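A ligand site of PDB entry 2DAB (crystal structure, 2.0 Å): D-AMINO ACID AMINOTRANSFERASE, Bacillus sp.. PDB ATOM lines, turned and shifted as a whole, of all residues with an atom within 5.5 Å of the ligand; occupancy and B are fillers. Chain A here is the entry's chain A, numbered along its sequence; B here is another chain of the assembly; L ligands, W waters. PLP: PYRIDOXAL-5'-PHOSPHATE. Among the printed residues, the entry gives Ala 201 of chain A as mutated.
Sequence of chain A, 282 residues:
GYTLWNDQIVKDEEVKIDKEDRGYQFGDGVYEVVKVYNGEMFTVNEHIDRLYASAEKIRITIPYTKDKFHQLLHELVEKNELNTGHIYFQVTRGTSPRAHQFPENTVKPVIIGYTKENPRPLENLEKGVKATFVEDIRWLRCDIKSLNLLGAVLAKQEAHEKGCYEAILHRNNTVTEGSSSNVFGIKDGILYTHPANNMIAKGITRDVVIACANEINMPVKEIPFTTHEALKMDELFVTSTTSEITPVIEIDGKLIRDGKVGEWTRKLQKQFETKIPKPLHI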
ATOM      1  N   TYR A  31     -11.265  28.801 -18.859  1.00  0.00           N
ATOM      2  CA  TYR A  31     -11.840  29.765 -19.812  1.00  0.00           C
ATOM      3  C   TYR A  31     -11.924  29.236 -21.257  1.00  0.00           C
ATOM      4  O   TYR A  31     -11.355  28.200 -21.575  1.00  0.00           O
ATOM      5  CB  TYR A  31     -10.985  31.055 -19.826  1.00  0.00           C
ATOM      6  CG  TYR A  31      -9.692  30.916 -20.605  1.00  0.00           C
ATOM      7  CD1 TYR A  31      -8.595  30.245 -20.060  1.00  0.00           C
ATOM      8  CD2 TYR A  31      -9.601  31.386 -21.919  1.00  0.00           C
ATOM      9  CE1 TYR A  31      -7.452  30.038 -20.796  1.00  0.00           C
ATOM     10  CE2 TYR A  31      -8.452  31.186 -22.669  1.00  0.00           C
ATOM     11  CZ  TYR A  31      -7.382  30.517 -22.100  1.00  0.00           C
ATOM     12  OH  TYR A  31      -6.225  30.355 -22.818  1.00  0.00           O
ATOM     13  N   GLU A  32     -12.606  30.001 -22.109  1.00  0.00           N
ATOM     14  CA  GLU A  32     -12.762  29.685 -23.523  1.00  0.00           C
ATOM     15  C   GLU A  32     -12.847  30.998 -24.283  1.00  0.00           C
ATOM     16  O   GLU A  32     -13.041  32.068 -23.681  1.00  0.00           O
ATOM     17  CB  GLU A  32     -14.062  28.904 -23.789  1.00  0.00           C
ATOM     18  CG  GLU A  32     -13.993  27.437 -23.459  1.00  0.00           C
ATOM     19  CD  GLU A  32     -12.997  26.699 -24.334  1.00  0.00           C
ATOM     20  OE1 GLU A  32     -12.829  27.059 -25.510  1.00  0.00           O
ATOM     21  OE2 GLU A  32     -12.360  25.769 -23.832  1.00  0.00           O
ATOM     22  N   VAL A  33     -12.601  30.919 -25.594  1.00  0.00           N
ATOM     23  CA  VAL A  33     -12.689  32.062 -26.494  1.00  0.00           C
ATOM     24  C   VAL A  33     -13.455  31.497 -27.679  1.00  0.00           C
ATOM     25  O   VAL A  33     -13.152  30.390 -28.145  1.00  0.00           O
ATOM     26  CB  VAL A  33     -11.309  32.589 -26.942  1.00  0.00           C
ATOM     27  CG1 VAL A  33     -11.468  33.709 -27.938  1.00  0.00           C
ATOM     28  CG2 VAL A  33     -10.522  33.097 -25.751  1.00  0.00           C
ATOM     29  N   HIS A  47     -16.690  24.463 -28.078  1.00  0.00           N
ATOM     30  CA  HIS A  47     -16.039  25.261 -27.056  1.00  0.00           C
ATOM     31  C   HIS A  47     -16.717  25.079 -25.713  1.00  0.00           C
ATOM     32  O   HIS A  47     -16.054  25.062 -24.691  1.00  0.00           O
ATOM     33  CB  HIS A  47     -16.022  26.735 -27.436  1.00  0.00           C
ATOM     34  CG  HIS A  47     -15.020  27.074 -28.492  1.00  0.00           C
ATOM     35  ND1 HIS A  47     -13.684  27.246 -28.232  1.00  0.00           N
ATOM     36  CD2 HIS A  47     -15.181  27.300 -29.809  1.00  0.00           C
ATOM     37  CE1 HIS A  47     -13.052  27.578 -29.347  1.00  0.00           C
ATOM     38  NE2 HIS A  47     -13.946  27.609 -30.325  1.00  0.00           N
ATOM     39  N   ARG A  50     -15.707  21.842 -24.353  1.00  0.00           N
ATOM     40  CA  ARG A  50     -14.384  21.935 -23.780  1.00  0.00           C
ATOM     41  C   ARG A  50     -14.355  22.688 -22.441  1.00  0.00           C
ATOM     42  O   ARG A  50     -13.591  22.328 -21.559  1.00  0.00           O
ATOM     43  CB  ARG A  50     -13.389  22.550 -24.761  1.00  0.00           C
ATOM     44  CG  ARG A  50     -11.944  22.291 -24.338  1.00  0.00           C
ATOM     45  CD  ARG A  50     -10.936  22.718 -25.391  1.00  0.00           C
ATOM     46  NE  ARG A  50     -11.044  24.138 -25.687  1.00  0.00           N
ATOM     47  CZ  ARG A  50     -10.213  24.812 -26.468  1.00  0.00           C
ATOM     48  NH1 ARG A  50      -9.198  24.193 -27.052  1.00  0.00           N
ATOM     49  NH2 ARG A  50     -10.388  26.109 -26.650  1.00  0.00           N
ATOM     50  N   ARG A 138       6.266  25.326 -18.836  1.00  0.00           N
ATOM     51  CA  ARG A 138       4.950  25.209 -18.219  1.00  0.00           C
ATOM     52  C   ARG A 138       4.731  23.935 -17.426  1.00  0.00           C
ATOM     53  O   ARG A 138       5.588  23.052 -17.397  1.00  0.00           O
ATOM     54  CB  ARG A 138       3.870  25.371 -19.287  1.00  0.00           C
ATOM     55  CG  ARG A 138       3.943  26.698 -20.018  1.00  0.00           C
ATOM     56  CD  ARG A 138       2.901  26.765 -21.100  1.00  0.00           C
ATOM     57  NE  ARG A 138       3.097  25.740 -22.125  1.00  0.00           N
ATOM     58  CZ  ARG A 138       2.161  25.319 -22.950  1.00  0.00           C
ATOM     59  NH1 ARG A 138       0.938  25.829 -22.901  1.00  0.00           N
ATOM     60  NH2 ARG A 138       2.445  24.391 -23.866  1.00  0.00           N
ATOM     61  N   LYS A 145      -7.491  23.921 -19.996  1.00  0.00           N
ATOM     62  CA  LYS A 145      -7.475  25.332 -20.390  1.00  0.00           C
ATOM     63  C   LYS A 145      -7.759  26.197 -19.138  1.00  0.00           C
ATOM     64  O   LYS A 145      -8.846  26.762 -18.982  1.00  0.00           O
ATOM     65  CB  LYS A 145      -8.553  25.601 -21.468  1.00  0.00           C
ATOM     66  CG  LYS A 145      -8.055  25.608 -22.921  1.00  0.00           C
ATOM     67  CD  LYS A 145      -8.321  26.938 -23.677  1.00  0.00           C
ATOM     68  CE  LYS A 145      -7.397  27.042 -24.908  1.00  0.00           C
ATOM     69  NZ  LYS A 145      -7.267  28.330 -25.577  1.00  0.00           N
ATOM     70  N   LEU A 149      -1.838  31.138 -16.571  1.00  0.00           N
ATOM     71  CA  LEU A 149      -1.196  31.427 -17.856  1.00  0.00           C
ATOM     72  C   LEU A 149       0.099  32.214 -17.845  1.00  0.00           C
ATOM     73  O   LEU A 149       0.527  32.715 -18.880  1.00  0.00           O
ATOM     74  CB  LEU A 149      -2.221  32.150 -18.759  1.00  0.00           C
ATOM     75  CG  LEU A 149      -3.463  31.361 -19.168  1.00  0.00           C
ATOM     76  CD1 LEU A 149      -4.563  32.288 -19.613  1.00  0.00           C
ATOM     77  CD2 LEU A 149      -3.122  30.381 -20.288  1.00  0.00           C
ATOM     78  N   GLU A 177       3.449  23.278 -28.763  1.00  0.00           N
ATOM     79  CA  GLU A 177       2.395  24.117 -29.322  1.00  0.00           C
ATOM     80  C   GLU A 177       2.888  25.546 -29.201  1.00  0.00           C
ATOM     81  O   GLU A 177       4.037  25.772 -28.861  1.00  0.00           O
ATOM     82  CB  GLU A 177       1.074  23.928 -28.542  1.00  0.00           C
ATOM     83  CG  GLU A 177       1.137  24.356 -27.049  1.00  0.00           C
ATOM     84  CD  GLU A 177      -0.120  24.026 -26.269  1.00  0.00           C
ATOM     85  OE1 GLU A 177      -1.195  23.837 -26.870  1.00  0.00           O
ATOM     86  OE2 GLU A 177      -0.025  23.928 -25.032  1.00  0.00           O
ATOM     87  N   GLY A 178       2.044  26.508 -29.544  1.00  0.00           N
ATOM     88  CA  GLY A 178       2.443  27.896 -29.419  1.00  0.00           C
ATOM     89  C   GLY A 178       1.909  28.450 -28.108  1.00  0.00           C
ATOM     90  O   GLY A 178       1.132  27.759 -27.441  1.00  0.00           O
ATOM     91  N   SER A 179       2.252  29.685 -27.759  1.00  0.00           N
ATOM     92  CA  SER A 179       1.786  30.267 -26.493  1.00  0.00           C
ATOM     93  C   SER A 179       0.265  30.416 -26.414  1.00  0.00           C
ATOM     94  O   SER A 179      -0.303  30.445 -25.315  1.00  0.00           O
ATOM     95  CB  SER A 179       2.496  31.577 -26.163  1.00  0.00           C
ATOM     96  OG  SER A 179       2.207  32.603 -27.079  1.00  0.00           O
ATOM     97  N   SER A 180      -0.396  30.493 -27.559  1.00  0.00           N
ATOM     98  CA  SER A 180      -1.849  30.574 -27.608  1.00  0.00           C
ATOM     99  C   SER A 180      -2.376  29.939 -28.902  1.00  0.00           C
ATOM    100  O   SER A 180      -3.422  30.311 -29.413  1.00  0.00           O
ATOM    101  CB  SER A 180      -2.312  32.032 -27.495  1.00  0.00           C
ATOM    102  OG  SER A 180      -1.732  32.821 -28.511  1.00  0.00           O
ATOM    103  N   SER A 181      -1.653  28.934 -29.402  1.00  0.00           N
ATOM    104  CA  SER A 181      -2.049  28.282 -30.624  1.00  0.00           C
ATOM    105  C   SER A 181      -1.428  26.900 -30.743  1.00  0.00           C
ATOM    106  O   SER A 181      -0.626  26.493 -29.891  1.00  0.00           O
ATOM    107  CB  SER A 181      -1.630  29.141 -31.832  1.00  0.00           C
ATOM    108  OG  SER A 181      -0.227  29.372 -31.836  1.00  0.00           O
ATOM    109  N   ASN A 182      -1.867  26.142 -31.737  1.00  0.00           N
ATOM    110  CA  ASN A 182      -1.291  24.829 -31.980  1.00  0.00           C
ATOM    111  C   ASN A 182      -0.368  24.966 -33.194  1.00  0.00           C
ATOM    112  O   ASN A 182      -0.568  25.853 -34.012  1.00  0.00           O
ATOM    113  CB  ASN A 182      -2.392  23.775 -32.181  1.00  0.00           C
ATOM    114  CG  ASN A 182      -3.069  23.387 -30.869  1.00  0.00           C
ATOM    115  OD1 ASN A 182      -4.253  23.644 -30.680  1.00  0.00           O
ATOM    116  ND2 ASN A 182      -2.320  22.778 -29.963  1.00  0.00           N
ATOM    117  N   ALA A 201      -2.765  21.875 -25.435  1.00  0.00           N
ATOM    118  CA  ALA A 201      -4.191  22.144 -25.380  1.00  0.00           C
ATOM    119  C   ALA A 201      -4.764  21.501 -26.642  1.00  0.00           C
ATOM    120  O   ALA A 201      -4.186  21.616 -27.719  1.00  0.00           O
ATOM    121  CB  ALA A 201      -4.443  23.644 -25.404  1.00  0.00           C
ATOM    122  N   LYS A 202      -5.868  20.781 -26.513  1.00  0.00           N
ATOM    123  CA  LYS A 202      -6.484  20.160 -27.682  1.00  0.00           C
ATOM    124  C   LYS A 202      -7.334  21.237 -28.320  1.00  0.00           C
ATOM    125  O   LYS A 202      -8.531  21.338 -28.047  1.00  0.00           O
ATOM    126  CB  LYS A 202      -7.320  18.941 -27.276  1.00  0.00           C
ATOM    127  CG  LYS A 202      -7.759  18.057 -28.435  1.00  0.00           C
ATOM    128  CD  LYS A 202      -8.410  16.788 -27.937  1.00  0.00           C
ATOM    129  CE  LYS A 202      -8.776  15.847 -29.066  1.00  0.00           C
ATOM    130  NZ  LYS A 202      -9.924  16.344 -29.847  1.00  0.00           N
ATOM    131  N   GLY A 203      -6.686  22.070 -29.130  1.00  0.00           N
ATOM    132  CA  GLY A 203      -7.377  23.144 -29.789  1.00  0.00           C
ATOM    133  C   GLY A 203      -8.565  22.729 -30.625  1.00  0.00           C
ATOM    134  O   GLY A 203      -8.577  21.658 -31.237  1.00  0.00           O
ATOM    135  N   ILE A 204      -9.554  23.599 -30.672  1.00  0.00           N
ATOM    136  CA  ILE A 204     -10.758  23.345 -31.447  1.00  0.00           C
ATOM    137  C   ILE A 204     -10.463  23.678 -32.909  1.00  0.00           C
ATOM    138  O   ILE A 204     -10.915  22.984 -33.809  1.00  0.00           O
ATOM    139  CB  ILE A 204     -11.944  24.110 -30.815  1.00  0.00           C
ATOM    140  CG1 ILE A 204     -12.313  23.411 -29.502  1.00  0.00           C
ATOM    141  CG2 ILE A 204     -13.156  24.148 -31.749  1.00  0.00           C
ATOM    142  CD1 ILE A 204     -13.367  24.061 -28.717  1.00  0.00           C
ATOM    143  N   THR A 205      -9.619  24.682 -33.125  1.00  0.00           N
ATOM    144  CA  THR A 205      -9.224  25.066 -34.469  1.00  0.00           C
ATOM    145  C   THR A 205      -8.369  23.934 -35.046  1.00  0.00           C
ATOM    146  O   THR A 205      -8.562  23.538 -36.194  1.00  0.00           O
ATOM    147  CB  THR A 205      -8.438  26.377 -34.453  1.00  0.00           C
ATOM    148  OG1 THR A 205      -9.189  27.352 -33.724  1.00  0.00           O
ATOM    149  CG2 THR A 205      -8.228  26.891 -35.873  1.00  0.00           C
ATOM    150  N   ARG A 206      -7.452  23.418 -34.239  1.00  0.00           N
ATOM    151  CA  ARG A 206      -6.572  22.304 -34.602  1.00  0.00           C
ATOM    152  C   ARG A 206      -7.389  21.124 -35.108  1.00  0.00           C
ATOM    153  O   ARG A 206      -7.042  20.529 -36.135  1.00  0.00           O
ATOM    154  CB  ARG A 206      -5.780  21.862 -33.360  1.00  0.00           C
ATOM    155  CG  ARG A 206      -5.047  20.548 -33.453  1.00  0.00           C
ATOM    156  CD  ARG A 206      -4.713  20.081 -32.064  1.00  0.00           C
ATOM    157  NE  ARG A 206      -3.820  18.918 -32.055  1.00  0.00           N
ATOM    158  CZ  ARG A 206      -4.230  17.655 -32.058  1.00  0.00           C
ATOM    159  NH1 ARG A 206      -5.521  17.366 -32.092  1.00  0.00           N
ATOM    160  NH2 ARG A 206      -3.331  16.675 -32.065  1.00  0.00           N
ATOM    161  N   THR A 239      -2.449  27.473 -35.415  1.00  0.00           N
ATOM    162  CA  THR A 239      -3.899  27.598 -35.388  1.00  0.00           C
ATOM    163  C   THR A 239      -4.424  28.063 -34.008  1.00  0.00           C
ATOM    164  O   THR A 239      -3.877  27.700 -32.978  1.00  0.00           O
ATOM    165  CB  THR A 239      -4.576  26.233 -35.670  1.00  0.00           C
ATOM    166  OG1 THR A 239      -4.076  25.265 -34.739  1.00  0.00           O
ATOM    167  CG2 THR A 239      -4.276  25.742 -37.068  1.00  0.00           C
ATOM    168  N   SER A 240      -5.472  28.879 -34.027  1.00  0.00           N
ATOM    169  CA  SER A 240      -6.141  29.330 -32.808  1.00  0.00           C
ATOM    170  C   SER A 240      -7.434  29.971 -33.266  1.00  0.00           C
ATOM    171  O   SER A 240      -7.598  30.279 -34.446  1.00  0.00           O
ATOM    172  CB  SER A 240      -5.275  30.308 -32.000  1.00  0.00           C
ATOM    173  OG  SER A 240      -5.469  31.645 -32.426  1.00  0.00           O
ATOM    174  N   THR A 241      -8.409  30.007 -32.365  1.00  0.00           N
ATOM    175  CA  THR A 241      -9.721  30.593 -32.613  1.00  0.00           C
ATOM    176  C   THR A 241      -9.657  31.993 -33.228  1.00  0.00           C
ATOM    177  O   THR A 241     -10.537  32.400 -33.980  1.00  0.00           O
ATOM    178  CB  THR A 241     -10.517  30.680 -31.294  1.00  0.00           C
ATOM    179  OG1 THR A 241     -10.827  29.358 -30.841  1.00  0.00           O
ATOM    180  CG2 THR A 241     -11.819  31.458 -31.486  1.00  0.00           C
ATOM    181  N   THR A 242      -8.644  32.761 -32.829  1.00  0.00           N
ATOM    182  CA  THR A 242      -8.468  34.120 -33.329  1.00  0.00           C
ATOM    183  C   THR A 242      -7.494  34.226 -34.501  1.00  0.00           C
ATOM    184  O   THR A 242      -7.663  35.059 -35.386  1.00  0.00           O
ATOM    185  CB  THR A 242      -8.031  35.053 -32.187  1.00  0.00           C
ATOM    186  OG1 THR A 242      -6.979  34.438 -31.446  1.00  0.00           O
ATOM    187  CG2 THR A 242      -9.188  35.310 -31.236  1.00  0.00           C
ATOM    188  N   HIS B 100      -2.093  38.500 -24.008  1.00  0.00           N
ATOM    189  CA  HIS B 100      -1.002  37.790 -23.330  1.00  0.00           C
ATOM    190  C   HIS B 100       0.268  38.608 -23.050  1.00  0.00           C
ATOM    191  O   HIS B 100       0.879  38.434 -22.011  1.00  0.00           O
ATOM    192  CB  HIS B 100      -0.585  36.529 -24.103  1.00  0.00           C
ATOM    193  CG  HIS B 100      -1.547  35.384 -23.998  1.00  0.00           C
ATOM    194  ND1 HIS B 100      -2.673  35.288 -24.777  1.00  0.00           N
ATOM    195  CD2 HIS B 100      -1.511  34.256 -23.256  1.00  0.00           C
ATOM    196  CE1 HIS B 100      -3.289  34.149 -24.525  1.00  0.00           C
ATOM    197  NE2 HIS B 100      -2.602  33.505 -23.603  1.00  0.00           N
HETATM  198  N1  PLP L   1      -2.866  26.304 -27.225  1.00  0.00           N
HETATM  199  C2  PLP L   1      -2.981  26.934 -26.008  1.00  0.00           C
HETATM  200  C2A PLP L   1      -1.871  26.814 -24.989  1.00  0.00           C
HETATM  201  C3  PLP L   1      -4.071  27.753 -25.737  1.00  0.00           C
HETATM  202  O3  PLP L   1      -4.143  28.377 -24.496  1.00  0.00           O
HETATM  203  C4  PLP L   1      -5.067  27.938 -26.703  1.00  0.00           C
HETATM  204  C4A PLP L   1      -6.190  28.735 -26.410  1.00  0.00           C
HETATM  205  C5  PLP L   1      -4.924  27.308 -27.944  1.00  0.00           C
HETATM  206  C6  PLP L   1      -3.843  26.483 -28.179  1.00  0.00           C
HETATM  207  C5A PLP L   1      -5.892  27.617 -29.106  1.00  0.00           C
HETATM  208  O4P PLP L   1      -6.930  26.690 -29.213  1.00  0.00           O
HETATM  209  P   PLP L   1      -8.189  27.085 -29.989  1.00  0.00           P
HETATM  210  O1P PLP L   1      -8.533  28.509 -29.762  1.00  0.00           O
HETATM  211  O2P PLP L   1      -9.123  26.112 -29.246  1.00  0.00           O
HETATM  212  O3P PLP L   1      -8.079  26.573 -31.363  1.00  0.00           O
HETATM  213  O   HOH W   1      -2.382  24.511 -23.055  1.00  0.00           O
HETATM  214  O   HOH W   2     -10.617  28.918 -27.680  1.00  0.00           O
HETATM  215  O   HOH W   3      -5.970  25.129 -32.263  1.00  0.00           O
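NZ of Lys 145 is covalently linked to C4A of the ligand, at 1.4 Å. The backbone NH (N) of Thr 241 lies close to an oxygen (O1P) of the ligand, 3.0 Å away. The side-chain hydroxyl of Thr 241 sits close to an oxygen (O1P) of the ligand, at 2.7 Å. An oxygen (O3P) of the ligand lies close to the backbone NH (N) of Thr 205 (3.0 Å). O3P of the ligand lies close to OG1 of Thr 205 (2.7 Å). An oxygen (O2P) of the ligand lies close to the guanidinium group (NH2) of Arg 50, at 2.9 Å. The backbone NH of Ile 204 lies close to an oxygen (O2P) of the ligand, at 2.9 Å. A nitrogen (N1) of the ligand lies close to the side-chain carboxylate (OE1) of Glu 177. The side-chain hydroxyl (OH) of Tyr 31 lies close to an oxygen (O3) of the ligand. A nitrogen (N1) of the ligand sits close to the backbone carbonyl oxygen (O) of Ser 181, 3.5 Å away.
Water W3 lies within hydrogen-bond range of OD1 of Asn 182 (2.8 Å), N of Arg 206 (3.0 Å) and OG1 of Thr 239 (3.1 Å). Water W2 lies within hydrogen-bond range of the backbone carbonyl oxygen of Val 33, the guanidinium group of Arg 50 and the side-chain hydroxyl of Thr 241.
OG1 of Thr 205 lies close to O of Ser 240 (3.4 Å). The guanidinium group (NE) of Arg 50 lies within salt-bridge range of the side-chain carboxylate (OE2) of Glu 32 (2.8 Å). OE1 of Glu 177 sits at hydrogen-bond distance from N of Ala 201 (2.9 Å). OE2 of Glu 177 is in salt-bridge range of NH2 of Arg 138 (2.8 Å). OE1 of Glu 177 sits at hydrogen-bond distance from ND2 of Asn 182. The backbone NH (N) of Gly 203 is in hydrogen-bond range of the side-chain amide oxygen (OD1) of Asn 182, 3.3 Å away. The side-chain amide nitrogen (ND2) of Asn 182 is in hydrogen-bond range of the backbone carbonyl oxygen (O) of Ala 201, at 3.1 Å. The backbone NH (N) of Asn 182 is in hydrogen-bond range of the backbone carbonyl oxygen (O) of Thr 239, at 2.8 Å.
Residues that only touch the ligand: Gly 203 (3.5 Å), Ala 201 (3.6 Å), Arg 138 (3.6 Å), Ser 180 (3.7 Å), Ser 240 (3.7 Å), Asn 182 (3.8 Å), Ser 179 (3.97 Å) and Gly 178 (3.99 Å). Hydrophobic or aromatic side chains that line the ligand: Ala 201 and Ile 204. Within 4 Å of the ligand: Tyr 31, Arg 50, Arg 138, Lys 145, Glu 177, Gly 178, Ser 179, Ser 180, Ser 181, Asn 182, Ala 201, Gly 203, Ile 204, Thr 205, Ser 240 and Thr 241. The nearest printed residue that does not touch the ligand is His 47 (4.2 Å).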
